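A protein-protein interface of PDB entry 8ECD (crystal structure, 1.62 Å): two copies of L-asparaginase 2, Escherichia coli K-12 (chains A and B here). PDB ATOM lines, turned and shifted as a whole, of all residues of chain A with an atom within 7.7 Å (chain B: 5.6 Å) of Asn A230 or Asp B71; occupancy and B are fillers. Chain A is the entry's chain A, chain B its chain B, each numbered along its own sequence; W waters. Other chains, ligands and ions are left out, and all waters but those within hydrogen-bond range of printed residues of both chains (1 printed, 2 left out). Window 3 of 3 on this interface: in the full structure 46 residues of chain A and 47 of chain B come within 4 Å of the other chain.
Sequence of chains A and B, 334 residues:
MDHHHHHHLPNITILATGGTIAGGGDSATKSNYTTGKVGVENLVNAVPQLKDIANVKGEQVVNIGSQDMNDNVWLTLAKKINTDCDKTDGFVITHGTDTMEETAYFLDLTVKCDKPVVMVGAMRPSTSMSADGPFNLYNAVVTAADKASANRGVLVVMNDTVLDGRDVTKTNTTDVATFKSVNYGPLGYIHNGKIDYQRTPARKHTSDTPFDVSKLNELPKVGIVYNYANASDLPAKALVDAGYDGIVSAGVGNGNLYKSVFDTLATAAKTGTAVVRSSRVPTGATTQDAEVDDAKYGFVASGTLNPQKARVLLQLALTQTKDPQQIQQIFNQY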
ATOM      1  N   ASN A 227     -30.174   3.574 -37.038  1.00  0.00           N
ATOM      2  CA  ASN A 227     -30.927   4.136 -35.927  1.00  0.00           C
ATOM      3  C   ASN A 227     -31.592   3.042 -35.115  1.00  0.00           C
ATOM      4  O   ASN A 227     -31.984   1.972 -35.669  1.00  0.00           O
ATOM      5  CB  ASN A 227     -31.984   5.169 -36.372  1.00  0.00           C
ATOM      6  CG  ASN A 227     -31.375   6.413 -36.954  1.00  0.00           C
ATOM      7  OD1 ASN A 227     -31.277   7.445 -36.263  1.00  0.00           O
ATOM      8  ND2 ASN A 227     -30.997   6.355 -38.226  1.00  0.00           N
ATOM      9  N   TYR A 228     -31.713   3.278 -33.812  1.00  0.00           N
ATOM     10  CA  TYR A 228     -32.148   2.320 -32.797  1.00  0.00           C
ATOM     11  C   TYR A 228     -32.239   3.165 -31.489  1.00  0.00           C
ATOM     12  O   TYR A 228     -31.879   4.361 -31.481  1.00  0.00           O
ATOM     13  CB  TYR A 228     -31.209   1.140 -32.686  1.00  0.00           C
ATOM     14  CG  TYR A 228     -29.753   1.533 -32.437  1.00  0.00           C
ATOM     15  CD1 TYR A 228     -28.945   1.885 -33.502  1.00  0.00           C
ATOM     16  CD2 TYR A 228     -29.198   1.510 -31.180  1.00  0.00           C
ATOM     17  CE1 TYR A 228     -27.641   2.250 -33.327  1.00  0.00           C
ATOM     18  CE2 TYR A 228     -27.879   1.886 -30.974  1.00  0.00           C
ATOM     19  CZ  TYR A 228     -27.104   2.245 -32.062  1.00  0.00           C
ATOM     20  OH  TYR A 228     -25.773   2.614 -32.040  1.00  0.00           O
ATOM     21  N   ALA A 229     -32.728   2.558 -30.435  1.00  0.00           N
ATOM     22  CA  ALA A 229     -32.851   3.246 -29.132  1.00  0.00           C
ATOM     23  C   ALA A 229     -31.441   3.610 -28.648  1.00  0.00           C
ATOM     24  O   ALA A 229     -30.504   2.824 -28.717  1.00  0.00           O
ATOM     25  CB  ALA A 229     -33.570   2.340 -28.168  1.00  0.00           C
ATOM     26  N   ASN A 230     -31.296   4.831 -28.152  1.00  0.00           N
ATOM     27  CA  ASN A 230     -30.034   5.297 -27.560  1.00  0.00           C
ATOM     28  C   ASN A 230     -28.925   5.280 -28.617  1.00  0.00           C
ATOM     29  O   ASN A 230     -27.747   5.057 -28.273  1.00  0.00           O
ATOM     30  CB  ASN A 230     -29.640   4.461 -26.367  1.00  0.00           C
ATOM     31  CG  ASN A 230     -28.914   5.274 -25.306  1.00  0.00           C
ATOM     32  OD1 ASN A 230     -27.808   5.833 -25.478  1.00  0.00           O
ATOM     33  ND2 ASN A 230     -29.585   5.369 -24.197  1.00  0.00           N
ATOM     34  N   ALA A 231     -29.257   5.549 -29.880  1.00  0.00           N
ATOM     35  CA  ALA A 231     -28.275   5.464 -30.955  1.00  0.00           C
ATOM     36  C   ALA A 231     -27.115   6.460 -30.715  1.00  0.00           C
ATOM     37  O   ALA A 231     -27.360   7.624 -30.489  1.00  0.00           O
ATOM     38  CB  ALA A 231     -28.886   5.713 -32.270  1.00  0.00           C
ATOM     39  N   SER A 232     -25.898   6.009 -30.954  1.00  0.00           N
ATOM     40  CA  SER A 232     -24.696   6.881 -30.886  1.00  0.00           C
ATOM     41  C   SER A 232     -24.648   7.778 -32.107  1.00  0.00           C
ATOM     42  O   SER A 232     -24.930   7.311 -33.241  1.00  0.00           O
ATOM     43  CB  SER A 232     -23.434   6.083 -30.868  1.00  0.00           C
ATOM     44  OG  SER A 232     -22.265   6.913 -30.790  1.00  0.00           O
ATOM     45  N   ASP A 233     -24.252   9.057 -31.916  1.00  0.00           N
ATOM     46  CA  ASP A 233     -23.890   9.863 -33.029  1.00  0.00           C
ATOM     47  C   ASP A 233     -22.460   9.691 -33.597  1.00  0.00           C
ATOM     48  O   ASP A 233     -22.115  10.331 -34.600  1.00  0.00           O
ATOM     49  CB  ASP A 233     -24.175  11.398 -32.747  1.00  0.00           C
ATOM     50  CG  ASP A 233     -23.272  11.938 -31.642  1.00  0.00           C
ATOM     51  OD1 ASP A 233     -22.323  11.237 -31.219  1.00  0.00           O
ATOM     52  OD2 ASP A 233     -23.557  13.099 -31.209  1.00  0.00           O
ATOM     53  N   TYR A 258     -32.959   8.996 -34.451  1.00  0.00           N
ATOM     54  CA  TYR A 258     -32.701   9.272 -33.012  1.00  0.00           C
ATOM     55  C   TYR A 258     -32.160  10.710 -32.954  1.00  0.00           C
ATOM     56  O   TYR A 258     -31.389  11.142 -33.791  1.00  0.00           O
ATOM     57  CB  TYR A 258     -31.708   8.258 -32.498  1.00  0.00           C
ATOM     58  CG  TYR A 258     -31.385   8.409 -31.041  1.00  0.00           C
ATOM     59  CD1 TYR A 258     -32.294   8.028 -30.099  1.00  0.00           C
ATOM     60  CD2 TYR A 258     -30.192   9.004 -30.609  1.00  0.00           C
ATOM     61  CE1 TYR A 258     -32.056   8.162 -28.745  1.00  0.00           C
ATOM     62  CE2 TYR A 258     -29.960   9.196 -29.262  1.00  0.00           C
ATOM     63  CZ  TYR A 258     -30.868   8.746 -28.328  1.00  0.00           C
ATOM     64  OH  TYR A 258     -30.679   8.828 -26.945  1.00  0.00           O
ATOM     65  N   SER A 260     -29.853  12.530 -31.507  1.00  0.00           N
ATOM     66  CA  SER A 260     -28.430  12.938 -31.669  1.00  0.00           C
ATOM     67  C   SER A 260     -27.946  12.648 -33.090  1.00  0.00           C
ATOM     68  O   SER A 260     -27.177  13.440 -33.660  1.00  0.00           O
ATOM     69  CB  SER A 260     -27.562  12.331 -30.649  1.00  0.00           C
ATOM     70  OG  SER A 260     -27.465  10.997 -30.871  1.00  0.00           O
ATOM     71  N   VAL A 261     -28.500  11.580 -33.727  1.00  0.00           N
ATOM     72  CA  VAL A 261     -28.178  11.327 -35.175  1.00  0.00           C
ATOM     73  C   VAL A 261     -28.781  12.436 -36.015  1.00  0.00           C
ATOM     74  O   VAL A 261     -28.127  12.954 -36.918  1.00  0.00           O
ATOM     75  CB  VAL A 261     -28.655   9.908 -35.562  1.00  0.00           C
ATOM     76  CG1 VAL A 261     -28.414   9.651 -37.031  1.00  0.00           C
ATOM     77  CG2 VAL A 261     -27.988   8.856 -34.730  1.00  0.00           C
ATOM     78  N   MET B  69     -36.389   6.801 -27.854  1.00  0.00           N
ATOM     79  CA  MET B  69     -36.311   5.857 -26.745  1.00  0.00           C
ATOM     80  C   MET B  69     -34.836   5.693 -26.324  1.00  0.00           C
ATOM     81  O   MET B  69     -33.916   5.820 -27.148  1.00  0.00           O
ATOM     82  CB  MET B  69     -36.950   4.530 -27.164  1.00  0.00           C
ATOM     83  CG  MET B  69     -37.065   3.498 -26.151  1.00  0.00           C
ATOM     84  SD  MET B  69     -37.974   4.070 -24.651  1.00  0.00           S
ATOM     85  CE  MET B  69     -39.484   4.725 -25.280  1.00  0.00           C
ATOM     86  N   ASN B  70     -34.617   5.411 -25.065  1.00  0.00           N
ATOM     87  CA  ASN B  70     -33.240   5.335 -24.536  1.00  0.00           C
ATOM     88  C   ASN B  70     -33.137   4.447 -23.299  1.00  0.00           C
ATOM     89  O   ASN B  70     -34.122   3.974 -22.779  1.00  0.00           O
ATOM     90  CB  ASN B  70     -32.709   6.757 -24.296  1.00  0.00           C
ATOM     91  CG  ASN B  70     -33.477   7.433 -23.194  1.00  0.00           C
ATOM     92  OD1 ASN B  70     -33.603   6.929 -22.088  1.00  0.00           O
ATOM     93  ND2 ASN B  70     -34.123   8.503 -23.549  1.00  0.00           N
ATOM     94  N   ASP B  71     -31.895   4.192 -22.870  1.00  0.00           N
ATOM     95  CA  ASP B  71     -31.589   3.258 -21.802  1.00  0.00           C
ATOM     96  C   ASP B  71     -32.294   3.706 -20.473  1.00  0.00           C
ATOM     97  O   ASP B  71     -32.698   2.848 -19.701  1.00  0.00           O
ATOM     98  CB  ASP B  71     -30.105   3.181 -21.488  1.00  0.00           C
ATOM     99  CG  ASP B  71     -29.195   2.584 -22.581  1.00  0.00           C
ATOM    100  OD1 ASP B  71     -29.687   2.070 -23.624  1.00  0.00           O
ATOM    101  OD2 ASP B  71     -27.993   2.709 -22.432  1.00  0.00           O
ATOM    102  N   ASN B  72     -32.362   5.023 -20.250  1.00  0.00           N
ATOM    103  CA  ASN B  72     -32.937   5.542 -18.968  1.00  0.00           C
ATOM    104  C   ASN B  72     -34.413   5.164 -18.862  1.00  0.00           C
ATOM    105  O   ASN B  72     -34.889   4.746 -17.794  1.00  0.00           O
ATOM    106  CB  ASN B  72     -32.733   7.036 -18.829  1.00  0.00           C
ATOM    107  CG  ASN B  72     -31.280   7.338 -18.526  1.00  0.00           C
ATOM    108  OD1 ASN B  72     -30.581   6.530 -17.925  1.00  0.00           O
ATOM    109  ND2 ASN B  72     -30.828   8.504 -18.918  1.00  0.00           N
ATOM    110  N   VAL B  73     -35.159   5.313 -19.965  1.00  0.00           N
ATOM    111  CA  VAL B  73     -36.576   4.923 -19.970  1.00  0.00           C
ATOM    112  C   VAL B  73     -36.708   3.435 -19.789  1.00  0.00           C
ATOM    113  O   VAL B  73     -37.599   3.001 -19.033  1.00  0.00           O
ATOM    114  CB  VAL B  73     -37.247   5.399 -21.261  1.00  0.00           C
ATOM    115  CG1 VAL B  73     -38.708   4.951 -21.268  1.00  0.00           C
ATOM    116  CG2 VAL B  73     -37.152   6.887 -21.475  1.00  0.00           C
ATOM    117  N   TRP B  74     -35.869   2.613 -20.458  1.00  0.00           N
ATOM    118  CA  TRP B  74     -35.933   1.134 -20.264  1.00  0.00           C
ATOM    119  C   TRP B  74     -35.785   0.791 -18.777  1.00  0.00           C
ATOM    120  O   TRP B  74     -36.535  -0.048 -18.243  1.00  0.00           O
ATOM    121  CB  TRP B  74     -34.842   0.459 -21.075  1.00  0.00           C
ATOM    122  CG  TRP B  74     -35.168   0.437 -22.538  1.00  0.00           C
ATOM    123  CD1 TRP B  74     -36.280   0.962 -23.166  1.00  0.00           C
ATOM    124  CD2 TRP B  74     -34.323  -0.096 -23.571  1.00  0.00           C
ATOM    125  NE1 TRP B  74     -36.212   0.711 -24.514  1.00  0.00           N
ATOM    126  CE2 TRP B  74     -35.041   0.055 -24.781  1.00  0.00           C
ATOM    127  CE3 TRP B  74     -33.034  -0.656 -23.584  1.00  0.00           C
ATOM    128  CZ2 TRP B  74     -34.458  -0.314 -26.006  1.00  0.00           C
ATOM    129  CZ3 TRP B  74     -32.512  -1.141 -24.764  1.00  0.00           C
ATOM    130  CH2 TRP B  74     -33.239  -0.932 -25.958  1.00  0.00           C
ATOM    131  N   LEU B  75     -34.742   1.363 -18.149  1.00  0.00           N
ATOM    132  CA  LEU B  75     -34.474   1.049 -16.742  1.00  0.00           C
ATOM    133  C   LEU B  75     -35.650   1.507 -15.850  1.00  0.00           C
ATOM    134  O   LEU B  75     -36.000   0.717 -14.936  1.00  0.00           O
ATOM    135  CB  LEU B  75     -33.168   1.729 -16.336  1.00  0.00           C
ATOM    136  CG  LEU B  75     -31.912   1.067 -16.892  1.00  0.00           C
ATOM    137  CD1 LEU B  75     -30.747   2.026 -16.680  1.00  0.00           C
ATOM    138  CD2 LEU B  75     -31.668  -0.278 -16.312  1.00  0.00           C
ATOM    139  N   THR B  76     -36.230   2.662 -16.128  1.00  0.00           N
ATOM    140  CA  THR B  76     -37.398   3.164 -15.374  1.00  0.00           C
ATOM    141  C   THR B  76     -38.510   2.146 -15.475  1.00  0.00           C
ATOM    142  O   THR B  76     -39.193   1.850 -14.480  1.00  0.00           O
ATOM    143  CB  THR B  76     -37.791   4.517 -15.887  1.00  0.00           C
ATOM    144  OG1 THR B  76     -36.706   5.398 -15.643  1.00  0.00           O
ATOM    145  CG2 THR B  76     -39.060   5.063 -15.268  1.00  0.00           C
ATOM    146  N   GLU B 218     -27.220   2.673 -15.435  1.00  0.00           N
ATOM    147  CA  GLU B 218     -26.796   2.756 -16.821  1.00  0.00           C
ATOM    148  C   GLU B 218     -26.516   1.395 -17.295  1.00  0.00           C
ATOM    149  O   GLU B 218     -26.361   0.438 -16.553  1.00  0.00           O
ATOM    150  CB  GLU B 218     -25.518   3.646 -16.997  1.00  0.00           C
ATOM    151  CG  GLU B 218     -24.400   3.140 -16.239  1.00  0.00           C
ATOM    152  CD  GLU B 218     -23.591   4.350 -15.801  1.00  0.00           C
ATOM    153  OE1 GLU B 218     -23.796   4.790 -14.654  1.00  0.00           O
ATOM    154  OE2 GLU B 218     -22.883   4.941 -16.658  1.00  0.00           O
ATOM    155  N   LEU B 219     -26.437   1.265 -18.630  1.00  0.00           N
ATOM    156  CA  LEU B 219     -26.167  -0.010 -19.313  1.00  0.00           C
ATOM    157  C   LEU B 219     -24.882   0.151 -20.122  1.00  0.00           C
ATOM    158  O   LEU B 219     -24.569   1.248 -20.592  1.00  0.00           O
ATOM    159  CB  LEU B 219     -27.347  -0.325 -20.264  1.00  0.00           C
ATOM    160  CG  LEU B 219     -28.698  -0.652 -19.607  1.00  0.00           C
ATOM    161  CD1 LEU B 219     -29.826  -0.640 -20.629  1.00  0.00           C
ATOM    162  CD2 LEU B 219     -28.654  -1.944 -18.826  1.00  0.00           C
ATOM    163  N   PRO B 220     -24.192  -0.981 -20.360  1.00  0.00           N
ATOM    164  CA  PRO B 220     -23.019  -1.021 -21.187  1.00  0.00           C
ATOM    165  C   PRO B 220     -23.315  -0.345 -22.539  1.00  0.00           C
ATOM    166  O   PRO B 220     -24.403  -0.484 -23.114  1.00  0.00           O
ATOM    167  CB  PRO B 220     -22.737  -2.502 -21.310  1.00  0.00           C
ATOM    168  CG  PRO B 220     -23.220  -3.070 -20.031  1.00  0.00           C
ATOM    169  CD  PRO B 220     -24.488  -2.299 -19.811  1.00  0.00           C
ATOM    170  N   VAL B 222     -23.293  -0.066 -26.304  1.00  0.00           N
ATOM    171  CA  VAL B 222     -23.320  -1.007 -27.463  1.00  0.00           C
ATOM    172  C   VAL B 222     -23.866  -0.233 -28.649  1.00  0.00           C
ATOM    173  O   VAL B 222     -24.936   0.361 -28.574  1.00  0.00           O
ATOM    174  CB  VAL B 222     -24.146  -2.263 -27.184  1.00  0.00           C
ATOM    175  CG1 VAL B 222     -24.303  -3.073 -28.473  1.00  0.00           C
ATOM    176  CG2 VAL B 222     -23.584  -3.071 -26.031  1.00  0.00           C
ATOM    177  N   TYR B 244     -16.254   1.611 -26.704  1.00  0.00           N
ATOM    178  CA  TYR B 244     -17.538   0.887 -26.548  1.00  0.00           C
ATOM    179  C   TYR B 244     -17.326  -0.484 -25.944  1.00  0.00           C
ATOM    180  O   TYR B 244     -16.376  -1.254 -26.208  1.00  0.00           O
ATOM    181  CB  TYR B 244     -18.325   0.866 -27.864  1.00  0.00           C
ATOM    182  CG  TYR B 244     -19.338   1.961 -27.971  1.00  0.00           C
ATOM    183  CD1 TYR B 244     -19.008   3.299 -27.766  1.00  0.00           C
ATOM    184  CD2 TYR B 244     -20.692   1.673 -28.192  1.00  0.00           C
ATOM    185  CE1 TYR B 244     -19.957   4.316 -27.813  1.00  0.00           C
ATOM    186  CE2 TYR B 244     -21.651   2.674 -28.263  1.00  0.00           C
ATOM    187  CZ  TYR B 244     -21.281   4.010 -28.088  1.00  0.00           C
ATOM    188  OH  TYR B 244     -22.222   4.977 -28.128  1.00  0.00           O
ATOM    189  N   ARG B 311     -28.489  -5.943 -29.853  1.00  0.00           N
ATOM    190  CA  ARG B 311     -27.939  -4.930 -28.978  1.00  0.00           C
ATOM    191  C   ARG B 311     -28.489  -5.065 -27.572  1.00  0.00           C
ATOM    192  O   ARG B 311     -27.764  -4.974 -26.580  1.00  0.00           O
ATOM    193  CB  ARG B 311     -28.163  -3.533 -29.508  1.00  0.00           C
ATOM    194  CG  ARG B 311     -27.982  -2.409 -28.459  1.00  0.00           C
ATOM    195  CD  ARG B 311     -28.041  -1.042 -29.081  1.00  0.00           C
ATOM    196  NE  ARG B 311     -27.756  -0.055 -27.993  1.00  0.00           N
ATOM    197  CZ  ARG B 311     -28.651   0.438 -27.182  1.00  0.00           C
ATOM    198  NH1 ARG B 311     -29.894   0.069 -27.266  1.00  0.00           N
ATOM    199  NH2 ARG B 311     -28.277   1.295 -26.233  1.00  0.00           N
ATOM    200  N   GLN B 315     -26.064  -5.781 -24.424  1.00  0.00           N
ATOM    201  CA  GLN B 315     -25.945  -4.869 -23.259  1.00  0.00           C
ATOM    202  C   GLN B 315     -26.126  -5.675 -21.981  1.00  0.00           C
ATOM    203  O   GLN B 315     -25.358  -5.498 -20.980  1.00  0.00           O
ATOM    204  CB  GLN B 315     -26.930  -3.745 -23.335  1.00  0.00           C
ATOM    205  CG  GLN B 315     -26.721  -2.699 -24.384  1.00  0.00           C
ATOM    206  CD  GLN B 315     -27.741  -1.587 -24.197  1.00  0.00           C
ATOM    207  OE1 GLN B 315     -28.905  -1.806 -24.442  1.00  0.00           O
ATOM    208  NE2 GLN B 315     -27.311  -0.415 -23.750  1.00  0.00           N
HETATM  209  O   HOH W   1     -32.876   9.878 -25.782  1.00  0.00           O
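Among the printed residues, merely in contact across the chains: Tyr A258 with Met B69 (3.4 Å), Asn A230 with Asn B70 (3.4 Å), Ala A229 with Met B69 (3.4 Å), Asn A230 with Arg B311 (3.4 Å), Tyr A228 with Arg B311 (3.5 Å), Ala A229 with Trp B74 (3.5 Å) and Tyr A258 with Asn B70 (3.9 Å).
No position is printed for both chains. Of the 11 pairs that touch across the chains among the printed residues, none has its exchanged pair printed and touching as well.
Water W1 lies within hydrogen-bond range of the side-chain hydroxyl (OH) of Tyr A258 (2.7 Å) and the side-chain amide nitrogen (ND2) of Asn B70 (2.9 Å).
OG of Ser A232 lies close to OH of Tyr B244, at 3.3 Å. The side-chain amide nitrogen (ND2) of Asn A230 lies close to the backbone NH (N) of Asp B71, 2.9 Å away. The guanidinium group of Arg B311 lies within hydrogen-bond range of the backbone carbonyl oxygen of Ala A229 (3.2 Å). The backbone carbonyl oxygen (O) of Met B69 is in hydrogen-bond range of the backbone NH (N) of Asn A230, 3.0 Å away.
Of the printed residues of chain B, Tyr A228 touches Arg B311 (3.5 Å). Asn A230 touches just these residues of chain B: Met B69 (3.0 Å), Asn B70 (3.4 Å), Asp B71 (2.9 Å) and Arg B311 (3.4 Å). Ala A231 touches none of the printed residues of chain B. Printed residues of chain B within 4 Å of Ser A232: Tyr B244 (3.2 Å). Of the printed residues of chain A, Met B69 touches Ala A229, Asn A230 and Tyr A258. Of the printed residues of chain A, Asn B70 touches Asn A230 (3.4 Å) and Tyr A258 (3.9 Å). Of chain A, only Asn A230 comes within 4 Å of Asp B71. Printed residues of chain A within 4 Å of Trp B74: Ala A229 (3.5 Å).
Of the 10 printed residues of chain A, 5 touch a printed residue of chain B. Hydrophobic or aromatic side chains of chain A that line the printed part of chain B: Tyr A228, Ala A229 and Tyr A258. Printed residues of chain B that touch a printed residue of chain A: Met B69, Asn B70, Asp B71, Trp B74, Tyr B244 and Arg B311. Among the printed residues, no Asp or Glu carboxylate lies within 4 Å of a Lys or Arg side-chain nitrogen of the other chain.
OD1 of Asp B71 is in salt-bridge range of NH2 of Arg B311 (3.1 Å). The side-chain amide oxygen (OD1) of Asn B70 lies within hydrogen-bond range of the backbone NH (N) of Asn B72, at 2.9 Å. The guanidinium group (NH2) of Arg B311 lies close to the side-chain amide nitrogen (NE2) of Gln B315, at 3.2 Å. O of Val B222 is in hydrogen-bond range of NE of Arg B311, at 2.9 Å. SD of Met B69 sits close to NE1 of Trp B74 (3.8 Å). The side-chain amide oxygen (OD1) of Asn A227 is in hydrogen-bond range of the backbone NH (N) of Tyr A258 (2.9 Å).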
